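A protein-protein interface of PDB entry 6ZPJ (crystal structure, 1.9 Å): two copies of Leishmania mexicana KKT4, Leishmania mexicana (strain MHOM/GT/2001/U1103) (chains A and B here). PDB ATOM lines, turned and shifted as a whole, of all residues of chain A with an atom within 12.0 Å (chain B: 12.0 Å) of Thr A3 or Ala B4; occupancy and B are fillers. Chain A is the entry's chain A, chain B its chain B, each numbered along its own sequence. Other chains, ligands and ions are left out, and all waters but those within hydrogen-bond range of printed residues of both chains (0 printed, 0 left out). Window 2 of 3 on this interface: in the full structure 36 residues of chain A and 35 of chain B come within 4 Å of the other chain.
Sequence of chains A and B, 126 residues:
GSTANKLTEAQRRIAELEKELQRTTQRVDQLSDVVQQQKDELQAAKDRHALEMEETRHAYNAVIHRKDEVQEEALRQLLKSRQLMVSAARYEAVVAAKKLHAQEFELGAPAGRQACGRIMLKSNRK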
ATOM      1  N   GLY A   1     -34.482  -2.177  -7.977  1.00  0.00           N
ATOM      2  CA  GLY A   1     -35.565  -1.230  -8.258  1.00  0.00           C
ATOM      3  C   GLY A   1     -35.108   0.146  -8.646  1.00  0.00           C
ATOM      4  O   GLY A   1     -33.956   0.319  -8.922  1.00  0.00           O
ATOM      5  N   SER A   2     -35.996   1.130  -8.487  1.00  0.00           N
ATOM      6  CA  SER A   2     -35.671   2.520  -8.884  1.00  0.00           C
ATOM      7  C   SER A   2     -34.408   3.041  -8.184  1.00  0.00           C
ATOM      8  O   SER A   2     -33.682   3.767  -8.802  1.00  0.00           O
ATOM      9  CB  SER A   2     -36.845   3.413  -8.586  1.00  0.00           C
ATOM     10  OG  SER A   2     -37.296   3.234  -7.255  1.00  0.00           O
ATOM     11  N   THR A   3     -34.355   2.893  -6.861  1.00  0.00           N
ATOM     12  CA  THR A   3     -33.191   3.400  -6.100  1.00  0.00           C
ATOM     13  C   THR A   3     -31.888   2.817  -6.666  1.00  0.00           C
ATOM     14  O   THR A   3     -31.007   3.554  -6.974  1.00  0.00           O
ATOM     15  CB  THR A   3     -33.399   3.189  -4.603  1.00  0.00           C
ATOM     16  OG1 THR A   3     -34.705   3.673  -4.326  1.00  0.00           O
ATOM     17  CG2 THR A   3     -32.368   3.934  -3.784  1.00  0.00           C
ATOM     18  N   ALA A   4     -31.847   1.493  -6.763  1.00  0.00           N
ATOM     19  CA  ALA A   4     -30.654   0.837  -7.321  1.00  0.00           C
ATOM     20  C   ALA A   4     -30.353   1.318  -8.747  1.00  0.00           C
ATOM     21  O   ALA A   4     -29.218   1.467  -9.081  1.00  0.00           O
ATOM     22  CB  ALA A   4     -30.864  -0.655  -7.257  1.00  0.00           C
ATOM     23  N   ASN A   5     -31.411   1.486  -9.535  1.00  0.00           N
ATOM     24  CA  ASN A   5     -31.215   1.941 -10.930  1.00  0.00           C
ATOM     25  C   ASN A   5     -30.670   3.375 -10.988  1.00  0.00           C
ATOM     26  O   ASN A   5     -29.839   3.646 -11.775  1.00  0.00           O
ATOM     27  CB  ASN A   5     -32.490   1.751 -11.747  1.00  0.00           C
ATOM     28  CG  ASN A   5     -32.902   0.307 -11.900  1.00  0.00           C
ATOM     29  OD1 ASN A   5     -32.142  -0.589 -11.571  1.00  0.00           O
ATOM     30  ND2 ASN A   5     -34.111   0.086 -12.379  1.00  0.00           N
ATOM     31  N   LYS A   6     -31.212   4.209 -10.129  1.00  0.00           N
ATOM     32  CA  LYS A   6     -30.676   5.584 -10.077  1.00  0.00           C
ATOM     33  C   LYS A   6     -29.215   5.600  -9.606  1.00  0.00           C
ATOM     34  O   LYS A   6     -28.498   6.438  -9.978  1.00  0.00           O
ATOM     35  CB  LYS A   6     -31.532   6.420  -9.123  1.00  0.00           C
ATOM     36  CG  LYS A   6     -32.878   6.850  -9.694  1.00  0.00           C
ATOM     37  CD  LYS A   6     -33.817   7.440  -8.659  1.00  0.00           C
ATOM     38  CE  LYS A   6     -35.237   7.532  -9.175  1.00  0.00           C
ATOM     39  NZ  LYS A   6     -36.180   7.989  -8.132  1.00  0.00           N
ATOM     40  N   LEU A   7     -28.886   4.644  -8.749  1.00  0.00           N
ATOM     41  CA  LEU A   7     -27.470   4.578  -8.301  1.00  0.00           C
ATOM     42  C   LEU A   7     -26.584   4.126  -9.466  1.00  0.00           C
ATOM     43  O   LEU A   7     -25.575   4.702  -9.644  1.00  0.00           O
ATOM     44  CB  LEU A   7     -27.356   3.664  -7.072  1.00  0.00           C
ATOM     45  CG  LEU A   7     -25.937   3.315  -6.638  1.00  0.00           C
ATOM     46  CD1 LEU A   7     -25.203   4.549  -6.159  1.00  0.00           C
ATOM     47  CD2 LEU A   7     -25.964   2.271  -5.544  1.00  0.00           C
ATOM     48  N   THR A   8     -27.030   3.086 -10.176  1.00  0.00           N
ATOM     49  CA  THR A   8     -26.268   2.688 -11.372  1.00  0.00           C
ATOM     50  C   THR A   8     -26.101   3.853 -12.345  1.00  0.00           C
ATOM     51  O   THR A   8     -24.990   4.134 -12.803  1.00  0.00           O
ATOM     52  CB  THR A   8     -26.958   1.502 -12.047  1.00  0.00           C
ATOM     53  OG1 THR A   8     -27.030   0.438 -11.080  1.00  0.00           O
ATOM     54  CG2 THR A   8     -26.149   1.022 -13.260  1.00  0.00           C
ATOM     55  N   GLU A   9     -27.191   4.577 -12.620  1.00  0.00           N
ATOM     56  CA  GLU A   9     -27.116   5.759 -13.468  1.00  0.00           C
ATOM     57  C   GLU A   9     -26.101   6.777 -12.947  1.00  0.00           C
ATOM     58  O   GLU A   9     -25.350   7.356 -13.745  1.00  0.00           O
ATOM     59  CB  GLU A   9     -28.517   6.384 -13.607  1.00  0.00           C
ATOM     60  CG  GLU A   9     -29.458   5.424 -14.415  1.00  0.00           C
ATOM     61  CD  GLU A   9     -30.937   5.700 -14.193  1.00  0.00           C
ATOM     62  OE1 GLU A   9     -31.748   4.756 -14.365  1.00  0.00           O
ATOM     63  OE2 GLU A   9     -31.274   6.844 -13.811  1.00  0.00           O
ATOM     64  N   ALA A  10     -26.148   7.092 -11.631  1.00  0.00           N
ATOM     65  CA  ALA A  10     -25.218   8.044 -11.021  1.00  0.00           C
ATOM     66  C   ALA A  10     -23.780   7.563 -11.130  1.00  0.00           C
ATOM     67  O   ALA A  10     -22.885   8.361 -11.380  1.00  0.00           O
ATOM     68  CB  ALA A  10     -25.579   8.291  -9.552  1.00  0.00           C
ATOM     69  N   GLN A  11     -23.536   6.270 -10.928  1.00  0.00           N
ATOM     70  CA  GLN A  11     -22.187   5.719 -11.059  1.00  0.00           C
ATOM     71  C   GLN A  11     -21.662   5.882 -12.487  1.00  0.00           C
ATOM     72  O   GLN A  11     -20.495   6.244 -12.698  1.00  0.00           O
ATOM     73  CB  GLN A  11     -22.212   4.256 -10.609  1.00  0.00           C
ATOM     74  CG  GLN A  11     -22.398   4.154  -9.079  1.00  0.00           C
ATOM     75  CD  GLN A  11     -22.629   2.698  -8.621  1.00  0.00           C
ATOM     76  OE1 GLN A  11     -23.197   1.882  -9.350  1.00  0.00           O
ATOM     77  NE2 GLN A  11     -22.230   2.392  -7.407  1.00  0.00           N
ATOM     78  N   ARG A  12     -22.528   5.646 -13.473  1.00  0.00           N
ATOM     79  CA  ARG A  12     -22.115   5.909 -14.849  1.00  0.00           C
ATOM     80  C   ARG A  12     -21.784   7.382 -15.045  1.00  0.00           C
ATOM     81  O   ARG A  12     -20.785   7.718 -15.689  1.00  0.00           O
ATOM     82  CB  ARG A  12     -23.192   5.477 -15.844  1.00  0.00           C
ATOM     83  CG  ARG A  12     -22.839   5.956 -17.293  1.00  0.00           C
ATOM     84  CD  ARG A  12     -23.814   5.560 -18.400  1.00  0.00           C
ATOM     85  NE  ARG A  12     -23.303   6.073 -19.666  1.00  0.00           N
ATOM     86  CZ  ARG A  12     -22.979   5.335 -20.723  1.00  0.00           C
ATOM     87  NH1 ARG A  12     -23.181   4.033 -20.735  1.00  0.00           N
ATOM     88  NH2 ARG A  12     -22.496   5.926 -21.799  1.00  0.00           N
ATOM     89  N   ILE A  14     -20.769   9.600 -12.848  1.00  0.00           N
ATOM     90  CA  ILE A  14     -19.462   9.829 -12.229  1.00  0.00           C
ATOM     91  C   ILE A  14     -18.337   9.411 -13.179  1.00  0.00           C
ATOM     92  O   ILE A  14     -17.371  10.160 -13.360  1.00  0.00           O
ATOM     93  CB  ILE A  14     -19.372   9.092 -10.876  1.00  0.00           C
ATOM     94  CG1 ILE A  14     -20.325   9.775  -9.877  1.00  0.00           C
ATOM     95  CG2 ILE A  14     -17.940   9.145 -10.298  1.00  0.00           C
ATOM     96  CD1 ILE A  14     -20.527   9.029  -8.533  1.00  0.00           C
ATOM     97  N   GLY B   1     -23.597  -0.411   3.682  1.00  0.00           N
ATOM     98  CA  GLY B   1     -24.435   0.774   3.642  1.00  0.00           C
ATOM     99  C   GLY B   1     -25.627   0.612   2.714  1.00  0.00           C
ATOM    100  O   GLY B   1     -25.583  -0.182   1.767  1.00  0.00           O
ATOM    101  N   SER B   2     -26.686   1.378   2.969  1.00  0.00           N
ATOM    102  CA  SER B   2     -27.911   1.197   2.209  1.00  0.00           C
ATOM    103  C   SER B   2     -27.744   1.735   0.785  1.00  0.00           C
ATOM    104  O   SER B   2     -26.892   2.583   0.495  1.00  0.00           O
ATOM    105  CB  SER B   2     -29.087   1.880   2.907  1.00  0.00           C
ATOM    106  OG  SER B   2     -29.197   3.266   2.584  1.00  0.00           O
ATOM    107  N   THR B   3     -28.579   1.273  -0.132  1.00  0.00           N
ATOM    108  CA  THR B   3     -28.493   1.714  -1.535  1.00  0.00           C
ATOM    109  C   THR B   3     -28.843   3.204  -1.622  1.00  0.00           C
ATOM    110  O   THR B   3     -28.240   3.910  -2.348  1.00  0.00           O
ATOM    111  CB  THR B   3     -29.465   0.872  -2.364  1.00  0.00           C
ATOM    112  OG1 THR B   3     -29.143  -0.498  -2.139  1.00  0.00           O
ATOM    113  CG2 THR B   3     -29.413   1.189  -3.841  1.00  0.00           C
ATOM    114  N   ALA B   4     -29.829   3.575  -0.820  1.00  0.00           N
ATOM    115  CA  ALA B   4     -30.221   5.001  -0.801  1.00  0.00           C
ATOM    116  C   ALA B   4     -29.070   5.899  -0.335  1.00  0.00           C
ATOM    117  O   ALA B   4     -28.895   6.957  -0.874  1.00  0.00           O
ATOM    118  CB  ALA B   4     -31.490   5.228   0.003  1.00  0.00           C
ATOM    119  N   ASN B   5     -28.363   5.450   0.694  1.00  0.00           N
ATOM    120  CA  ASN B   5     -27.198   6.218   1.187  1.00  0.00           C
ATOM    121  C   ASN B   5     -26.114   6.333   0.123  1.00  0.00           C
ATOM    122  O   ASN B   5     -25.535   7.366  -0.028  1.00  0.00           O
ATOM    123  CB  ASN B   5     -26.638   5.611   2.468  1.00  0.00           C
ATOM    124  CG  ASN B   5     -27.538   5.796   3.669  1.00  0.00           C
ATOM    125  OD1 ASN B   5     -28.446   6.610   3.649  1.00  0.00           O
ATOM    126  ND2 ASN B   5     -27.283   5.040   4.720  1.00  0.00           N
ATOM    127  N   LYS B   6     -25.899   5.234  -0.588  1.00  0.00           N
ATOM    128  CA  LYS B   6     -24.918   5.241  -1.689  1.00  0.00           C
ATOM    129  C   LYS B   6     -25.341   6.251  -2.780  1.00  0.00           C
ATOM    130  O   LYS B   6     -24.503   6.898  -3.327  1.00  0.00           O
ATOM    131  CB  LYS B   6     -24.761   3.830  -2.275  1.00  0.00           C
ATOM    132  CG  LYS B   6     -24.089   2.766  -1.414  1.00  0.00           C
ATOM    133  CD  LYS B   6     -24.023   1.406  -2.092  1.00  0.00           C
ATOM    134  CE  LYS B   6     -23.955   0.241  -1.125  1.00  0.00           C
ATOM    135  NZ  LYS B   6     -24.075  -1.074  -1.800  1.00  0.00           N
ATOM    136  N   LEU B   7     -26.637   6.287  -3.060  1.00  0.00           N
ATOM    137  CA  LEU B   7     -27.136   7.230  -4.102  1.00  0.00           C
ATOM    138  C   LEU B   7     -26.883   8.677  -3.660  1.00  0.00           C
ATOM    139  O   LEU B   7     -26.521   9.469  -4.456  1.00  0.00           O
ATOM    140  CB  LEU B   7     -28.631   6.980  -4.334  1.00  0.00           C
ATOM    141  CG  LEU B   7     -29.336   7.910  -5.319  1.00  0.00           C
ATOM    142  CD1 LEU B   7     -28.673   7.870  -6.683  1.00  0.00           C
ATOM    143  CD2 LEU B   7     -30.806   7.557  -5.441  1.00  0.00           C
ATOM    144  N   THR B   8     -27.170   8.973  -2.391  1.00  0.00           N
ATOM    145  CA  THR B   8     -26.937  10.340  -1.862  1.00  0.00           C
ATOM    146  C   THR B   8     -25.461  10.697  -2.051  1.00  0.00           C
ATOM    147  O   THR B   8     -25.165  11.777  -2.531  1.00  0.00           O
ATOM    148  CB  THR B   8     -27.459  10.433  -0.420  1.00  0.00           C
ATOM    149  OG1 THR B   8     -28.862  10.179  -0.437  1.00  0.00           O
ATOM    150  CG2 THR B   8     -27.184  11.771   0.228  1.00  0.00           C
ATOM    151  N   GLU B   9     -24.571   9.778  -1.690  1.00  0.00           N
ATOM    152  CA  GLU B   9     -23.124  10.022  -1.830  1.00  0.00           C
ATOM    153  C   GLU B   9     -22.717  10.161  -3.308  1.00  0.00           C
ATOM    154  O   GLU B   9     -21.886  10.957  -3.594  1.00  0.00           O
ATOM    155  CB  GLU B   9     -22.366   8.905  -1.106  1.00  0.00           C
ATOM    156  CG  GLU B   9     -20.861   8.983  -1.215  1.00  0.00           C
ATOM    157  CD  GLU B   9     -20.229  10.312  -0.848  1.00  0.00           C
ATOM    158  OE1 GLU B   9     -20.773  11.019   0.009  1.00  0.00           O
ATOM    159  OE2 GLU B   9     -19.185  10.622  -1.424  1.00  0.00           O
ATOM    160  N   ALA B  10     -23.311   9.322  -4.164  1.00  0.00           N
ATOM    161  CA  ALA B  10     -23.009   9.456  -5.604  1.00  0.00           C
ATOM    162  C   ALA B  10     -23.473  10.828  -6.135  1.00  0.00           C
ATOM    163  O   ALA B  10     -22.791  11.391  -6.932  1.00  0.00           O
ATOM    164  CB  ALA B  10     -23.639   8.338  -6.357  1.00  0.00           C
ATOM    165  N   GLN B  11     -24.603  11.286  -5.619  1.00  0.00           N
ATOM    166  CA  GLN B  11     -25.133  12.584  -6.100  1.00  0.00           C
ATOM    167  C   GLN B  11     -24.220  13.732  -5.621  1.00  0.00           C
ATOM    168  O   GLN B  11     -23.991  14.643  -6.340  1.00  0.00           O
ATOM    169  CB  GLN B  11     -26.580  12.743  -5.647  1.00  0.00           C
ATOM    170  CG  GLN B  11     -27.582  11.878  -6.383  1.00  0.00           C
ATOM    171  CD  GLN B  11     -28.914  11.855  -5.675  1.00  0.00           C
ATOM    172  OE1 GLN B  11     -29.023  12.183  -4.502  1.00  0.00           O
ATOM    173  NE2 GLN B  11     -29.945  11.459  -6.391  1.00  0.00           N
ATOM    174  N   ARG B  12     -23.689  13.568  -4.422  1.00  0.00           N
ATOM    175  CA  ARG B  12     -22.722  14.568  -3.908  1.00  0.00           C
ATOM    176  C   ARG B  12     -21.469  14.612  -4.777  1.00  0.00           C
ATOM    177  O   ARG B  12     -20.974  15.654  -5.064  1.00  0.00           O
ATOM    178  CB  ARG B  12     -22.375  14.291  -2.433  1.00  0.00           C
ATOM    179  CG  ARG B  12     -21.684  15.412  -1.680  1.00  0.00           C
ATOM    180  CD  ARG B  12     -20.899  14.869  -0.504  1.00  0.00           C
ATOM    181  NE  ARG B  12     -19.912  13.858  -0.847  1.00  0.00           N
ATOM    182  CZ  ARG B  12     -18.764  14.081  -1.476  1.00  0.00           C
ATOM    183  NH1 ARG B  12     -18.422  15.299  -1.855  1.00  0.00           N
ATOM    184  NH2 ARG B  12     -17.951  13.079  -1.733  1.00  0.00           N
ATOM    185  N   ARG B  13     -20.983  13.415  -5.108  1.00  0.00           N
ATOM    186  CA  ARG B  13     -19.784  13.320  -5.947  1.00  0.00           C
ATOM    187  C   ARG B  13     -20.018  13.873  -7.359  1.00  0.00           C
ATOM    188  O   ARG B  13     -19.130  14.456  -7.878  1.00  0.00           O
ATOM    189  CB  ARG B  13     -19.348  11.859  -6.037  1.00  0.00           C
ATOM    190  CG  ARG B  13     -18.098  11.617  -6.861  1.00  0.00           C
ATOM    191  CD  ARG B  13     -16.857  12.150  -6.191  1.00  0.00           C
ATOM    192  NE  ARG B  13     -15.763  11.727  -7.037  1.00  0.00           N
ATOM    193  CZ  ARG B  13     -14.677  12.423  -7.309  1.00  0.00           C
ATOM    194  NH1 ARG B  13     -14.518  13.633  -6.809  1.00  0.00           N
ATOM    195  NH2 ARG B  13     -13.764  11.907  -8.112  1.00  0.00           N
ATOM    196  N   ILE B  14     -21.212  13.609  -7.890  1.00  0.00           N
ATOM    197  CA  ILE B  14     -21.524  14.241  -9.180  1.00  0.00           C
ATOM    198  C   ILE B  14     -21.402  15.761  -9.065  1.00  0.00           C
ATOM    199  O   ILE B  14     -20.807  16.415  -9.924  1.00  0.00           O
ATOM    200  CB  ILE B  14     -22.921  13.819  -9.682  1.00  0.00           C
ATOM    201  CG1 ILE B  14     -22.843  12.407 -10.247  1.00  0.00           C
ATOM    202  CG2 ILE B  14     -23.355  14.749 -10.884  1.00  0.00           C
ATOM    203  CD1 ILE B  14     -24.135  11.652 -10.478  1.00  0.00           C
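CG2 of Thr A3 touches CA of Ala B4, at 3.8 Å.
CG2 of Thr B3 touches CA of Ala A4, at 3.7 Å.
Lys A6 touches Leu B7.
Leu A7 touches Thr B3 (CD2 to CG2, 3.996 Å).
O of Lys B6 touches CD1 of Leu A7, 3.7 Å away.
N of Leu B7 touches CD1 of Leu A7, 3.8 Å away.
Ala A10 touches Ala B10 (CB to CB, 3.7 Å).
Ala A10 touches Ile B14 (O to CD1, 3.6 Å).
Arg B13 touches Ile A14 (CG to CD1, 3.9 Å).
CG1 of Ile B14 touches CG1 of Ile A14, 3.7 Å away.
Thr A3 touches just one residue of chain B: Ala B4.
Ala B4 touches one residue of chain A.
No residue of chain B comes within 4 Å of Gly A1.
Lys A6 touches one residue of chain B.
Ser B2 touches none of the printed residues of chain A.
Printed residues of chain A within 4 Å of Arg B13: Ile A14 (3.9 Å).
Of the printed residues of chain B, Leu A7 touches Thr B3, Lys B6 and Leu B7.
Glu B9 touches none of the printed residues of chain A.
OG1 of Thr A8 is in hydrogen-bond range of O of Ala A4 (3.1 Å).
The backbone NH (N) of Ala B4 lies close to the side-chain hydroxyl (OG) of Ser B2, 3.5 Å away.
The side-chain hydroxyl of Thr B8 is in hydrogen-bond range of the backbone carbonyl oxygen of Ala B4 (3.3 Å).
Printed residues of chain A that touch a printed residue of chain B: Thr A3, Ala A4, Lys A6, Leu A7, Ala A10 and Ile A14.
Of the 14 printed residues of chain B, 7 touch a printed residue of chain A.
Among the printed residues, no Asp or Glu carboxylate lies within 4 Å of a Lys or Arg side-chain nitrogen of the other chain.
Thr A3 touches Ala B4, and with the chains exchanged Ala A4 touches Thr B3.
Leu A7 touches Thr B3, but with the chains exchanged Thr A3 does not touch Leu B7 (4.3 Å).
Ala B10 touches its own counterpart, Ala A10.
Ala A10 touches Ile B14, and with the chains exchanged Ile A14 touches Ala B10.
Of the 11 pairs that touch across the chains among the printed residues, 9 have their exchanged pair printed and touching as well.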
